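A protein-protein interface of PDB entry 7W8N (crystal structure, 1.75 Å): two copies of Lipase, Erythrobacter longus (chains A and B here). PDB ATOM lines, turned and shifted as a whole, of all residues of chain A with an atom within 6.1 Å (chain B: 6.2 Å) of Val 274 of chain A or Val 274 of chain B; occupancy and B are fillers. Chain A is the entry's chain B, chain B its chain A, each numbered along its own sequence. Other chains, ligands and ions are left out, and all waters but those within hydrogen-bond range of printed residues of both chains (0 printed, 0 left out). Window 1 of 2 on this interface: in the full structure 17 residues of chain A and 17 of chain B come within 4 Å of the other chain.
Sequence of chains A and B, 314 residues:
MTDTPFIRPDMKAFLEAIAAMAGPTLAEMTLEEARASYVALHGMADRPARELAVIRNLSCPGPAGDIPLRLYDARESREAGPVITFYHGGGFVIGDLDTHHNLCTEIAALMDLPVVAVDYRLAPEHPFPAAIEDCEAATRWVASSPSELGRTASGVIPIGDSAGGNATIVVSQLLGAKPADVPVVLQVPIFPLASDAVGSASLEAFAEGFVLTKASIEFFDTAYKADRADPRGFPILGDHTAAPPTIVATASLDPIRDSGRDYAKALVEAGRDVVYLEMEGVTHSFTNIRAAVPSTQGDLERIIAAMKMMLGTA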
ATOM      1  N   PRO A 245      -2.919 -14.921  -7.705  1.00  0.00           N
ATOM      2  CA  PRO A 245      -2.663 -13.845  -8.673  1.00  0.00           C
ATOM      3  C   PRO A 245      -2.914 -14.347 -10.083  1.00  0.00           C
ATOM      4  O   PRO A 245      -2.573 -15.481 -10.422  1.00  0.00           O
ATOM      5  CB  PRO A 245      -1.185 -13.515  -8.455  1.00  0.00           C
ATOM      6  CG  PRO A 245      -0.918 -13.949  -7.050  1.00  0.00           C
ATOM      7  CD  PRO A 245      -1.734 -15.186  -6.873  1.00  0.00           C
ATOM      8  N   THR A 246      -3.536 -13.504 -10.896  1.00  0.00           N
ATOM      9  CA  THR A 246      -4.060 -13.922 -12.191  1.00  0.00           C
ATOM     10  C   THR A 246      -3.701 -12.944 -13.296  1.00  0.00           C
ATOM     11  O   THR A 246      -3.714 -11.720 -13.106  1.00  0.00           O
ATOM     12  CB  THR A 246      -5.580 -14.057 -12.136  1.00  0.00           C
ATOM     13  OG1 THR A 246      -5.929 -15.022 -11.152  1.00  0.00           O
ATOM     14  CG2 THR A 246      -6.144 -14.515 -13.478  1.00  0.00           C
ATOM     15  N   ILE A 247      -3.376 -13.498 -14.461  1.00  0.00           N
ATOM     16  CA  ILE A 247      -3.334 -12.742 -15.708  1.00  0.00           C
ATOM     17  C   ILE A 247      -4.379 -13.360 -16.623  1.00  0.00           C
ATOM     18  O   ILE A 247      -4.262 -14.529 -17.018  1.00  0.00           O
ATOM     19  CB  ILE A 247      -1.948 -12.772 -16.355  1.00  0.00           C
ATOM     20  CG1 ILE A 247      -0.908 -12.101 -15.445  1.00  0.00           C
ATOM     21  CG2 ILE A 247      -1.952 -12.109 -17.744  1.00  0.00           C
ATOM     22  CD1 ILE A 247       0.463 -12.532 -15.745  1.00  0.00           C
ATOM     23  N   VAL A 248      -5.400 -12.588 -16.974  1.00  0.00           N
ATOM     24  CA  VAL A 248      -6.404 -12.997 -17.946  1.00  0.00           C
ATOM     25  C   VAL A 248      -6.067 -12.279 -19.245  1.00  0.00           C
ATOM     26  O   VAL A 248      -6.000 -11.046 -19.279  1.00  0.00           O
ATOM     27  CB  VAL A 248      -7.829 -12.637 -17.486  1.00  0.00           C
ATOM     28  CG1 VAL A 248      -8.820 -13.023 -18.574  1.00  0.00           C
ATOM     29  CG2 VAL A 248      -8.194 -13.315 -16.195  1.00  0.00           C
ATOM     30  N   ALA A 264     -12.384 -11.986 -15.154  1.00  0.00           N
ATOM     31  CA  ALA A 264     -11.552 -10.933 -14.581  1.00  0.00           C
ATOM     32  C   ALA A 264     -12.393 -10.022 -13.680  1.00  0.00           C
ATOM     33  O   ALA A 264     -11.954  -9.652 -12.586  1.00  0.00           O
ATOM     34  CB  ALA A 264     -10.850 -10.149 -15.683  1.00  0.00           C
ATOM     35  N   LEU A 267     -12.925 -11.693 -10.318  1.00  0.00           N
ATOM     36  CA  LEU A 267     -11.762 -11.641  -9.437  1.00  0.00           C
ATOM     37  C   LEU A 267     -11.646 -10.282  -8.747  1.00  0.00           C
ATOM     38  O   LEU A 267     -11.335 -10.221  -7.549  1.00  0.00           O
ATOM     39  CB  LEU A 267     -10.487 -11.936 -10.221  1.00  0.00           C
ATOM     40  CG  LEU A 267     -10.324 -13.400 -10.661  1.00  0.00           C
ATOM     41  CD1 LEU A 267      -9.088 -13.573 -11.537  1.00  0.00           C
ATOM     42  CD2 LEU A 267     -10.211 -14.307  -9.484  1.00  0.00           C
ATOM     43  N   VAL A 268     -11.832  -9.197  -9.506  1.00  0.00           N
ATOM     44  CA  VAL A 268     -11.830  -7.852  -8.910  1.00  0.00           C
ATOM     45  C   VAL A 268     -12.918  -7.752  -7.848  1.00  0.00           C
ATOM     46  O   VAL A 268     -12.696  -7.233  -6.745  1.00  0.00           O
ATOM     47  CB  VAL A 268     -12.015  -6.772  -9.988  1.00  0.00           C
ATOM     48  CG1 VAL A 268     -12.127  -5.383  -9.335  1.00  0.00           C
ATOM     49  CG2 VAL A 268     -10.882  -6.754 -10.975  1.00  0.00           C
ATOM     50  N   ARG A 272      -9.279  -9.831  -5.607  1.00  0.00           N
ATOM     51  CA  ARG A 272      -8.069 -10.566  -5.963  1.00  0.00           C
ATOM     52  C   ARG A 272      -7.234  -9.782  -6.972  1.00  0.00           C
ATOM     53  O   ARG A 272      -7.767  -8.999  -7.757  1.00  0.00           O
ATOM     54  CB  ARG A 272      -8.432 -11.933  -6.543  1.00  0.00           C
ATOM     55  CG  ARG A 272      -9.526 -12.686  -5.752  1.00  0.00           C
ATOM     56  CD  ARG A 272      -9.158 -12.813  -4.297  1.00  0.00           C
ATOM     57  NE  ARG A 272      -7.897 -13.557  -4.113  1.00  0.00           N
ATOM     58  CZ  ARG A 272      -7.089 -13.423  -3.061  1.00  0.00           C
ATOM     59  NH1 ARG A 272      -7.384 -12.569  -2.078  1.00  0.00           N
ATOM     60  NH2 ARG A 272      -5.969 -14.135  -2.982  1.00  0.00           N
ATOM     61  N   ASP A 273      -5.919 -10.015  -6.969  1.00  0.00           N
ATOM     62  CA  ASP A 273      -5.030  -9.296  -7.884  1.00  0.00           C
ATOM     63  C   ASP A 273      -5.126  -9.898  -9.285  1.00  0.00           C
ATOM     64  O   ASP A 273      -4.998 -11.108  -9.457  1.00  0.00           O
ATOM     65  CB  ASP A 273      -3.572  -9.350  -7.431  1.00  0.00           C
ATOM     66  CG  ASP A 273      -3.332  -8.690  -6.079  1.00  0.00           C
ATOM     67  OD1 ASP A 273      -4.187  -7.904  -5.626  1.00  0.00           O
ATOM     68  OD2 ASP A 273      -2.252  -8.958  -5.497  1.00  0.00           O
ATOM     69  N   VAL A 274      -5.365  -9.056 -10.276  1.00  0.00           N
ATOM     70  CA  VAL A 274      -5.532  -9.551 -11.638  1.00  0.00           C
ATOM     71  C   VAL A 274      -5.029  -8.515 -12.631  1.00  0.00           C
ATOM     72  O   VAL A 274      -5.273  -7.309 -12.492  1.00  0.00           O
ATOM     73  CB  VAL A 274      -7.008  -9.928 -11.902  1.00  0.00           C
ATOM     74  CG1 VAL A 274      -7.926  -8.782 -11.538  1.00  0.00           C
ATOM     75  CG2 VAL A 274      -7.212 -10.319 -13.369  1.00  0.00           C
ATOM     76  N   VAL A 275      -4.343  -9.008 -13.662  1.00  0.00           N
ATOM     77  CA  VAL A 275      -3.999  -8.240 -14.838  1.00  0.00           C
ATOM     78  C   VAL A 275      -4.963  -8.688 -15.930  1.00  0.00           C
ATOM     79  O   VAL A 275      -5.048  -9.896 -16.215  1.00  0.00           O
ATOM     80  CB  VAL A 275      -2.541  -8.478 -15.254  1.00  0.00           C
ATOM     81  CG1 VAL A 275      -2.193  -7.675 -16.503  1.00  0.00           C
ATOM     82  CG2 VAL A 275      -1.599  -8.157 -14.111  1.00  0.00           C
ATOM     83  N   TYR A 276      -5.714  -7.734 -16.500  1.00  0.00           N
ATOM     84  CA  TYR A 276      -6.632  -7.995 -17.609  1.00  0.00           C
ATOM     85  C   TYR A 276      -6.055  -7.366 -18.882  1.00  0.00           C
ATOM     86  O   TYR A 276      -5.877  -6.139 -18.971  1.00  0.00           O
ATOM     87  CB  TYR A 276      -8.062  -7.491 -17.310  1.00  0.00           C
ATOM     88  CG  TYR A 276      -8.962  -7.804 -18.456  1.00  0.00           C
ATOM     89  CD1 TYR A 276      -9.361  -9.114 -18.692  1.00  0.00           C
ATOM     90  CD2 TYR A 276      -9.343  -6.822 -19.364  1.00  0.00           C
ATOM     91  CE1 TYR A 276     -10.120  -9.443 -19.780  1.00  0.00           C
ATOM     92  CE2 TYR A 276     -10.107  -7.149 -20.478  1.00  0.00           C
ATOM     93  CZ  TYR A 276     -10.499  -8.470 -20.667  1.00  0.00           C
ATOM     94  OH  TYR A 276     -11.229  -8.845 -21.786  1.00  0.00           O
ATOM     95  N   LEU A 277      -5.727  -8.205 -19.867  1.00  0.00           N
ATOM     96  CA  LEU A 277      -5.192  -7.729 -21.138  1.00  0.00           C
ATOM     97  C   LEU A 277      -6.099  -8.215 -22.253  1.00  0.00           C
ATOM     98  O   LEU A 277      -6.288  -9.427 -22.421  1.00  0.00           O
ATOM     99  CB  LEU A 277      -3.753  -8.200 -21.381  1.00  0.00           C
ATOM    100  CG  LEU A 277      -2.684  -7.807 -20.353  1.00  0.00           C
ATOM    101  CD1 LEU A 277      -1.357  -8.495 -20.726  1.00  0.00           C
ATOM    102  CD2 LEU A 277      -2.498  -6.312 -20.221  1.00  0.00           C
ATOM    103  N   MET A 310       4.267 -10.142 -12.331  1.00  0.00           N
ATOM    104  CA  MET A 310       3.434 -10.691 -11.272  1.00  0.00           C
ATOM    105  C   MET A 310       4.160 -11.737 -10.438  1.00  0.00           C
ATOM    106  O   MET A 310       3.709 -12.041  -9.326  1.00  0.00           O
ATOM    107  CB  MET A 310       2.155 -11.293 -11.840  1.00  0.00           C
ATOM    108  CG  MET A 310       1.204 -10.265 -12.457  1.00  0.00           C
ATOM    109  SD  MET A 310       0.519  -9.106 -11.241  1.00  0.00           S
ATOM    110  CE  MET A 310      -0.731 -10.141 -10.517  1.00  0.00           C
ATOM    111  N   PRO B 245      -4.483   2.699 -20.715  1.00  0.00           N
ATOM    112  CA  PRO B 245      -3.990   1.631 -19.837  1.00  0.00           C
ATOM    113  C   PRO B 245      -4.019   2.114 -18.403  1.00  0.00           C
ATOM    114  O   PRO B 245      -3.636   3.242 -18.126  1.00  0.00           O
ATOM    115  CB  PRO B 245      -2.561   1.406 -20.330  1.00  0.00           C
ATOM    116  CG  PRO B 245      -2.611   1.853 -21.785  1.00  0.00           C
ATOM    117  CD  PRO B 245      -3.501   3.056 -21.743  1.00  0.00           C
ATOM    118  N   THR B 246      -4.460   1.247 -17.498  1.00  0.00           N
ATOM    119  CA  THR B 246      -4.739   1.645 -16.124  1.00  0.00           C
ATOM    120  C   THR B 246      -4.123   0.686 -15.115  1.00  0.00           C
ATOM    121  O   THR B 246      -4.159  -0.537 -15.301  1.00  0.00           O
ATOM    122  CB  THR B 246      -6.242   1.691 -15.882  1.00  0.00           C
ATOM    123  OG1 THR B 246      -6.840   2.645 -16.777  1.00  0.00           O
ATOM    124  CG2 THR B 246      -6.534   2.135 -14.449  1.00  0.00           C
ATOM    125  N   ILE B 247      -3.622   1.246 -14.018  1.00  0.00           N
ATOM    126  CA  ILE B 247      -3.322   0.478 -12.807  1.00  0.00           C
ATOM    127  C   ILE B 247      -4.191   1.033 -11.694  1.00  0.00           C
ATOM    128  O   ILE B 247      -4.067   2.212 -11.355  1.00  0.00           O
ATOM    129  CB  ILE B 247      -1.840   0.575 -12.437  1.00  0.00           C
ATOM    130  CG1 ILE B 247      -0.958  -0.066 -13.503  1.00  0.00           C
ATOM    131  CG2 ILE B 247      -1.588  -0.048 -11.079  1.00  0.00           C
ATOM    132  CD1 ILE B 247       0.431   0.529 -13.510  1.00  0.00           C
ATOM    133  N   VAL B 248      -5.100   0.209 -11.172  1.00  0.00           N
ATOM    134  CA  VAL B 248      -5.931   0.570 -10.018  1.00  0.00           C
ATOM    135  C   VAL B 248      -5.351  -0.130  -8.800  1.00  0.00           C
ATOM    136  O   VAL B 248      -5.311  -1.360  -8.760  1.00  0.00           O
ATOM    137  CB  VAL B 248      -7.391   0.141 -10.196  1.00  0.00           C
ATOM    138  CG1 VAL B 248      -8.212   0.522  -8.909  1.00  0.00           C
ATOM    139  CG2 VAL B 248      -8.012   0.793 -11.451  1.00  0.00           C
ATOM    140  N   ALA B 264     -12.334  -0.722 -11.648  1.00  0.00           N
ATOM    141  CA  ALA B 264     -11.588  -1.716 -12.419  1.00  0.00           C
ATOM    142  C   ALA B 264     -12.526  -2.686 -13.133  1.00  0.00           C
ATOM    143  O   ALA B 264     -12.267  -3.072 -14.284  1.00  0.00           O
ATOM    144  CB  ALA B 264     -10.602  -2.469 -11.522  1.00  0.00           C
ATOM    145  N   LEU B 267     -13.733  -1.027 -16.279  1.00  0.00           N
ATOM    146  CA  LEU B 267     -12.735  -1.043 -17.330  1.00  0.00           C
ATOM    147  C   LEU B 267     -12.682  -2.410 -18.013  1.00  0.00           C
ATOM    148  O   LEU B 267     -12.616  -2.480 -19.241  1.00  0.00           O
ATOM    149  CB  LEU B 267     -11.362  -0.663 -16.776  1.00  0.00           C
ATOM    150  CG  LEU B 267     -11.177   0.790 -16.308  1.00  0.00           C
ATOM    151  CD1 LEU B 267      -9.780   1.061 -15.814  1.00  0.00           C
ATOM    152  CD2 LEU B 267     -11.489   1.759 -17.407  1.00  0.00           C
ATOM    153  N   VAL B 268     -12.708  -3.500 -17.245  1.00  0.00           N
ATOM    154  CA  VAL B 268     -12.746  -4.834 -17.857  1.00  0.00           C
ATOM    155  C   VAL B 268     -14.006  -4.986 -18.704  1.00  0.00           C
ATOM    156  O   VAL B 268     -13.970  -5.500 -19.830  1.00  0.00           O
ATOM    157  CB  VAL B 268     -12.673  -5.932 -16.788  1.00  0.00           C
ATOM    158  CG1 VAL B 268     -12.904  -7.316 -17.425  1.00  0.00           C
ATOM    159  CG2 VAL B 268     -11.341  -5.889 -16.003  1.00  0.00           C
ATOM    160  N   ARG B 272     -10.904  -2.793 -21.578  1.00  0.00           N
ATOM    161  CA  ARG B 272      -9.702  -1.985 -21.448  1.00  0.00           C
ATOM    162  C   ARG B 272      -8.655  -2.726 -20.629  1.00  0.00           C
ATOM    163  O   ARG B 272      -8.993  -3.516 -19.757  1.00  0.00           O
ATOM    164  CB  ARG B 272     -10.031  -0.646 -20.766  1.00  0.00           C
ATOM    165  CG  ARG B 272     -11.248   0.064 -21.338  1.00  0.00           C
ATOM    166  CD  ARG B 272     -11.154   0.223 -22.849  1.00  0.00           C
ATOM    167  NE  ARG B 272     -10.020   1.027 -23.265  1.00  0.00           N
ATOM    168  CZ  ARG B 272      -9.420   0.937 -24.450  1.00  0.00           C
ATOM    169  NH1 ARG B 272      -9.820   0.044 -25.358  1.00  0.00           N
ATOM    170  NH2 ARG B 272      -8.402   1.734 -24.729  1.00  0.00           N
ATOM    171  N   ASP B 273      -7.380  -2.434 -20.895  1.00  0.00           N
ATOM    172  CA  ASP B 273      -6.294  -3.109 -20.192  1.00  0.00           C
ATOM    173  C   ASP B 273      -6.165  -2.504 -18.803  1.00  0.00           C
ATOM    174  O   ASP B 273      -6.021  -1.284 -18.673  1.00  0.00           O
ATOM    175  CB  ASP B 273      -4.970  -2.942 -20.919  1.00  0.00           C
ATOM    176  CG  ASP B 273      -4.932  -3.645 -22.281  1.00  0.00           C
ATOM    177  OD1 ASP B 273      -5.799  -4.497 -22.572  1.00  0.00           O
ATOM    178  OD2 ASP B 273      -4.014  -3.329 -23.051  1.00  0.00           O
ATOM    179  N   VAL B 274      -6.151  -3.350 -17.784  1.00  0.00           N
ATOM    180  CA  VAL B 274      -6.091  -2.860 -16.402  1.00  0.00           C
ATOM    181  C   VAL B 274      -5.375  -3.866 -15.508  1.00  0.00           C
ATOM    182  O   VAL B 274      -5.547  -5.089 -15.623  1.00  0.00           O
ATOM    183  CB  VAL B 274      -7.501  -2.515 -15.864  1.00  0.00           C
ATOM    184  CG1 VAL B 274      -8.411  -3.690 -15.960  1.00  0.00           C
ATOM    185  CG2 VAL B 274      -7.418  -2.006 -14.396  1.00  0.00           C
ATOM    186  N   VAL B 275      -4.529  -3.328 -14.632  1.00  0.00           N
ATOM    187  CA  VAL B 275      -3.947  -4.061 -13.515  1.00  0.00           C
ATOM    188  C   VAL B 275      -4.703  -3.662 -12.267  1.00  0.00           C
ATOM    189  O   VAL B 275      -4.776  -2.467 -11.940  1.00  0.00           O
ATOM    190  CB  VAL B 275      -2.457  -3.751 -13.347  1.00  0.00           C
ATOM    191  CG1 VAL B 275      -1.892  -4.589 -12.190  1.00  0.00           C
ATOM    192  CG2 VAL B 275      -1.681  -4.000 -14.613  1.00  0.00           C
ATOM    193  N   TYR B 276      -5.285  -4.632 -11.584  1.00  0.00           N
ATOM    194  CA  TYR B 276      -5.991  -4.404 -10.328  1.00  0.00           C
ATOM    195  C   TYR B 276      -5.172  -5.040  -9.209  1.00  0.00           C
ATOM    196  O   TYR B 276      -4.993  -6.258  -9.200  1.00  0.00           O
ATOM    197  CB  TYR B 276      -7.405  -4.990 -10.356  1.00  0.00           C
ATOM    198  CG  TYR B 276      -8.097  -4.695  -9.047  1.00  0.00           C
ATOM    199  CD1 TYR B 276      -8.506  -3.402  -8.741  1.00  0.00           C
ATOM    200  CD2 TYR B 276      -8.245  -5.671  -8.078  1.00  0.00           C
ATOM    201  CE1 TYR B 276      -9.083  -3.105  -7.524  1.00  0.00           C
ATOM    202  CE2 TYR B 276      -8.817  -5.384  -6.858  1.00  0.00           C
ATOM    203  CZ  TYR B 276      -9.235  -4.091  -6.587  1.00  0.00           C
ATOM    204  OH  TYR B 276      -9.785  -3.795  -5.357  1.00  0.00           O
ATOM    205  N   LEU B 277      -4.708  -4.221  -8.260  1.00  0.00           N
ATOM    206  CA  LEU B 277      -3.926  -4.673  -7.116  1.00  0.00           C
ATOM    207  C   LEU B 277      -4.610  -4.206  -5.848  1.00  0.00           C
ATOM    208  O   LEU B 277      -4.777  -2.994  -5.647  1.00  0.00           O
ATOM    209  CB  LEU B 277      -2.502  -4.119  -7.138  1.00  0.00           C
ATOM    210  CG  LEU B 277      -1.623  -4.373  -8.365  1.00  0.00           C
ATOM    211  CD1 LEU B 277      -0.276  -3.692  -8.198  1.00  0.00           C
ATOM    212  CD2 LEU B 277      -1.470  -5.836  -8.602  1.00  0.00           C
ATOM    213  N   MET B 310       3.494  -1.830 -17.518  1.00  0.00           N
ATOM    214  CA  MET B 310       2.473  -1.284 -18.408  1.00  0.00           C
ATOM    215  C   MET B 310       3.030  -0.237 -19.350  1.00  0.00           C
ATOM    216  O   MET B 310       2.430  -0.012 -20.406  1.00  0.00           O
ATOM    217  CB  MET B 310       1.323  -0.694 -17.592  1.00  0.00           C
ATOM    218  CG  MET B 310       0.465  -1.768 -16.947  1.00  0.00           C
ATOM    219  SD  MET B 310      -0.335  -2.944 -18.072  1.00  0.00           S
ATOM    220  CE  MET B 310      -1.876  -2.041 -18.330  1.00  0.00           C
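N of Tyr 276 of chain A sits at hydrogen-bond distance from O of Val 274 of chain B, at 2.8 Å.
The backbone NH (N) of Tyr 276 of chain B is in hydrogen-bond range of the backbone carbonyl oxygen (O) of Val 274 of chain A.
Printed residues of chain B that touch a printed residue of chain A: Ala 264, Val 268, Arg 272, Asp 273, Val 274, Val 275, Tyr 276 and Leu 277.
Hydrophobic or aromatic side chains of chain B that line the printed part of chain A: Ala 264, Val 268 and Tyr 276.
Hydrophobic or aromatic side chains of chain A within 4 Å of the printed part of chain B: Ala 264, Val 268 and Tyr 276.
Among the printed residues, no Asp or Glu carboxylate lies within 4 Å of a Lys or Arg side-chain nitrogen of the other chain.
Val 274 of chain A touches just these residues of chain B: Val 274, Val 275 and Tyr 276.
Of the printed residues of chain A, Tyr 276 of chain B touches Val 268 (3.9 Å), Arg 272 (3.4 Å), Asp 273 (3.3 Å) and Val 274 (2.8 Å).
Of the printed residues of chain A, Asp 273 of chain B touches Tyr 276 and Leu 277.
Printed residues of chain B within 4 Å of Tyr 276 of chain A: Val 268, Arg 272, Asp 273 and Val 274.
Printed residues of chain B within 4 Å of Leu 277 of chain A: Asp 273 (3.6 Å).
Of the printed residues of chain B, Val 275 of chain A touches Val 274.
Pro 245 of chain B touches none of the printed residues of chain A.
Ile 247 of chain A touches none of the printed residues of chain B.
The nearest residue of chain B that does not touch Val 274 of chain A is Leu 277 of chain B (5.3 Å).
The nearest residue of chain A that does not touch Val 274 of chain B is Leu 277 of chain A (5.3 Å).
The nearest printed residue of chain A that does not touch Arg 272 of chain B is Leu 277 of chain A (5.7 Å).
Ala 264 of chain A touches Val 268 of chain B, and with the chains exchanged Val 268 of chain A touches Ala 264 of chain B.
Val 268 of chain A touches Tyr 276 of chain B, and with the chains exchanged Tyr 276 of chain A touches Val 268 of chain B.
Arg 272 of chain A touches Tyr 276 of chain B, and with the chains exchanged Tyr 276 of chain A touches Arg 272 of chain B.
Val 274 of chain A touches Val 275 of chain B, and with the chains exchanged Val 275 of chain A touches Val 274 of chain B.
Of the 15 pairs that touch across the chains among the printed residues, 15 have their exchanged pair printed and touching as well.
O of Val 248 of chain B lies within hydrogen-bond range of N of Leu 277 of chain B (3.0 Å).
The backbone NH (N) of Val 248 of chain B lies within hydrogen-bond range of the backbone carbonyl oxygen (O) of Val 275 of chain B, 2.8 Å away.
The backbone carbonyl oxygen (O) of Val 248 of chain A lies within hydrogen-bond range of the backbone NH (N) of Leu 277 of chain A (2.9 Å).
The backbone carbonyl oxygen (O) of Leu 267 of chain A lies within hydrogen-bond range of the backbone NH (N) of Arg 272 of chain A (2.9 Å).
The backbone NH (N) of Thr 246 of chain B is in hydrogen-bond range of the backbone carbonyl oxygen (O) of Asp 273 of chain B (3.2 Å).
N of Val 275 of chain B is in hydrogen-bond range of O of Thr 246 of chain B.
CG1 of Val 268 of chain B touches CB of Ala 264 of chain A, at 3.9 Å.
Val 268 of chain A touches Ala 264 of chain B.
Tyr 276 of chain B touches Val 268 of chain A.
CA of Asp 273 of chain A touches O of Tyr 276 of chain B (3.3 Å).
Asp 273 of chain A touches Leu 277 of chain B (OD1 to CA, 3.6 Å).
Val 274 of chain A touches Val 274 of chain B.
Val 275 of chain B touches Val 274 of chain A.
Val 275 of chain A touches Val 274 of chain B (CA to O, 3.6 Å).
Asp 273 of chain B touches Tyr 276 of chain A.
OD1 of Asp 273 of chain B touches CA of Leu 277 of chain A, at 3.6 Å.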
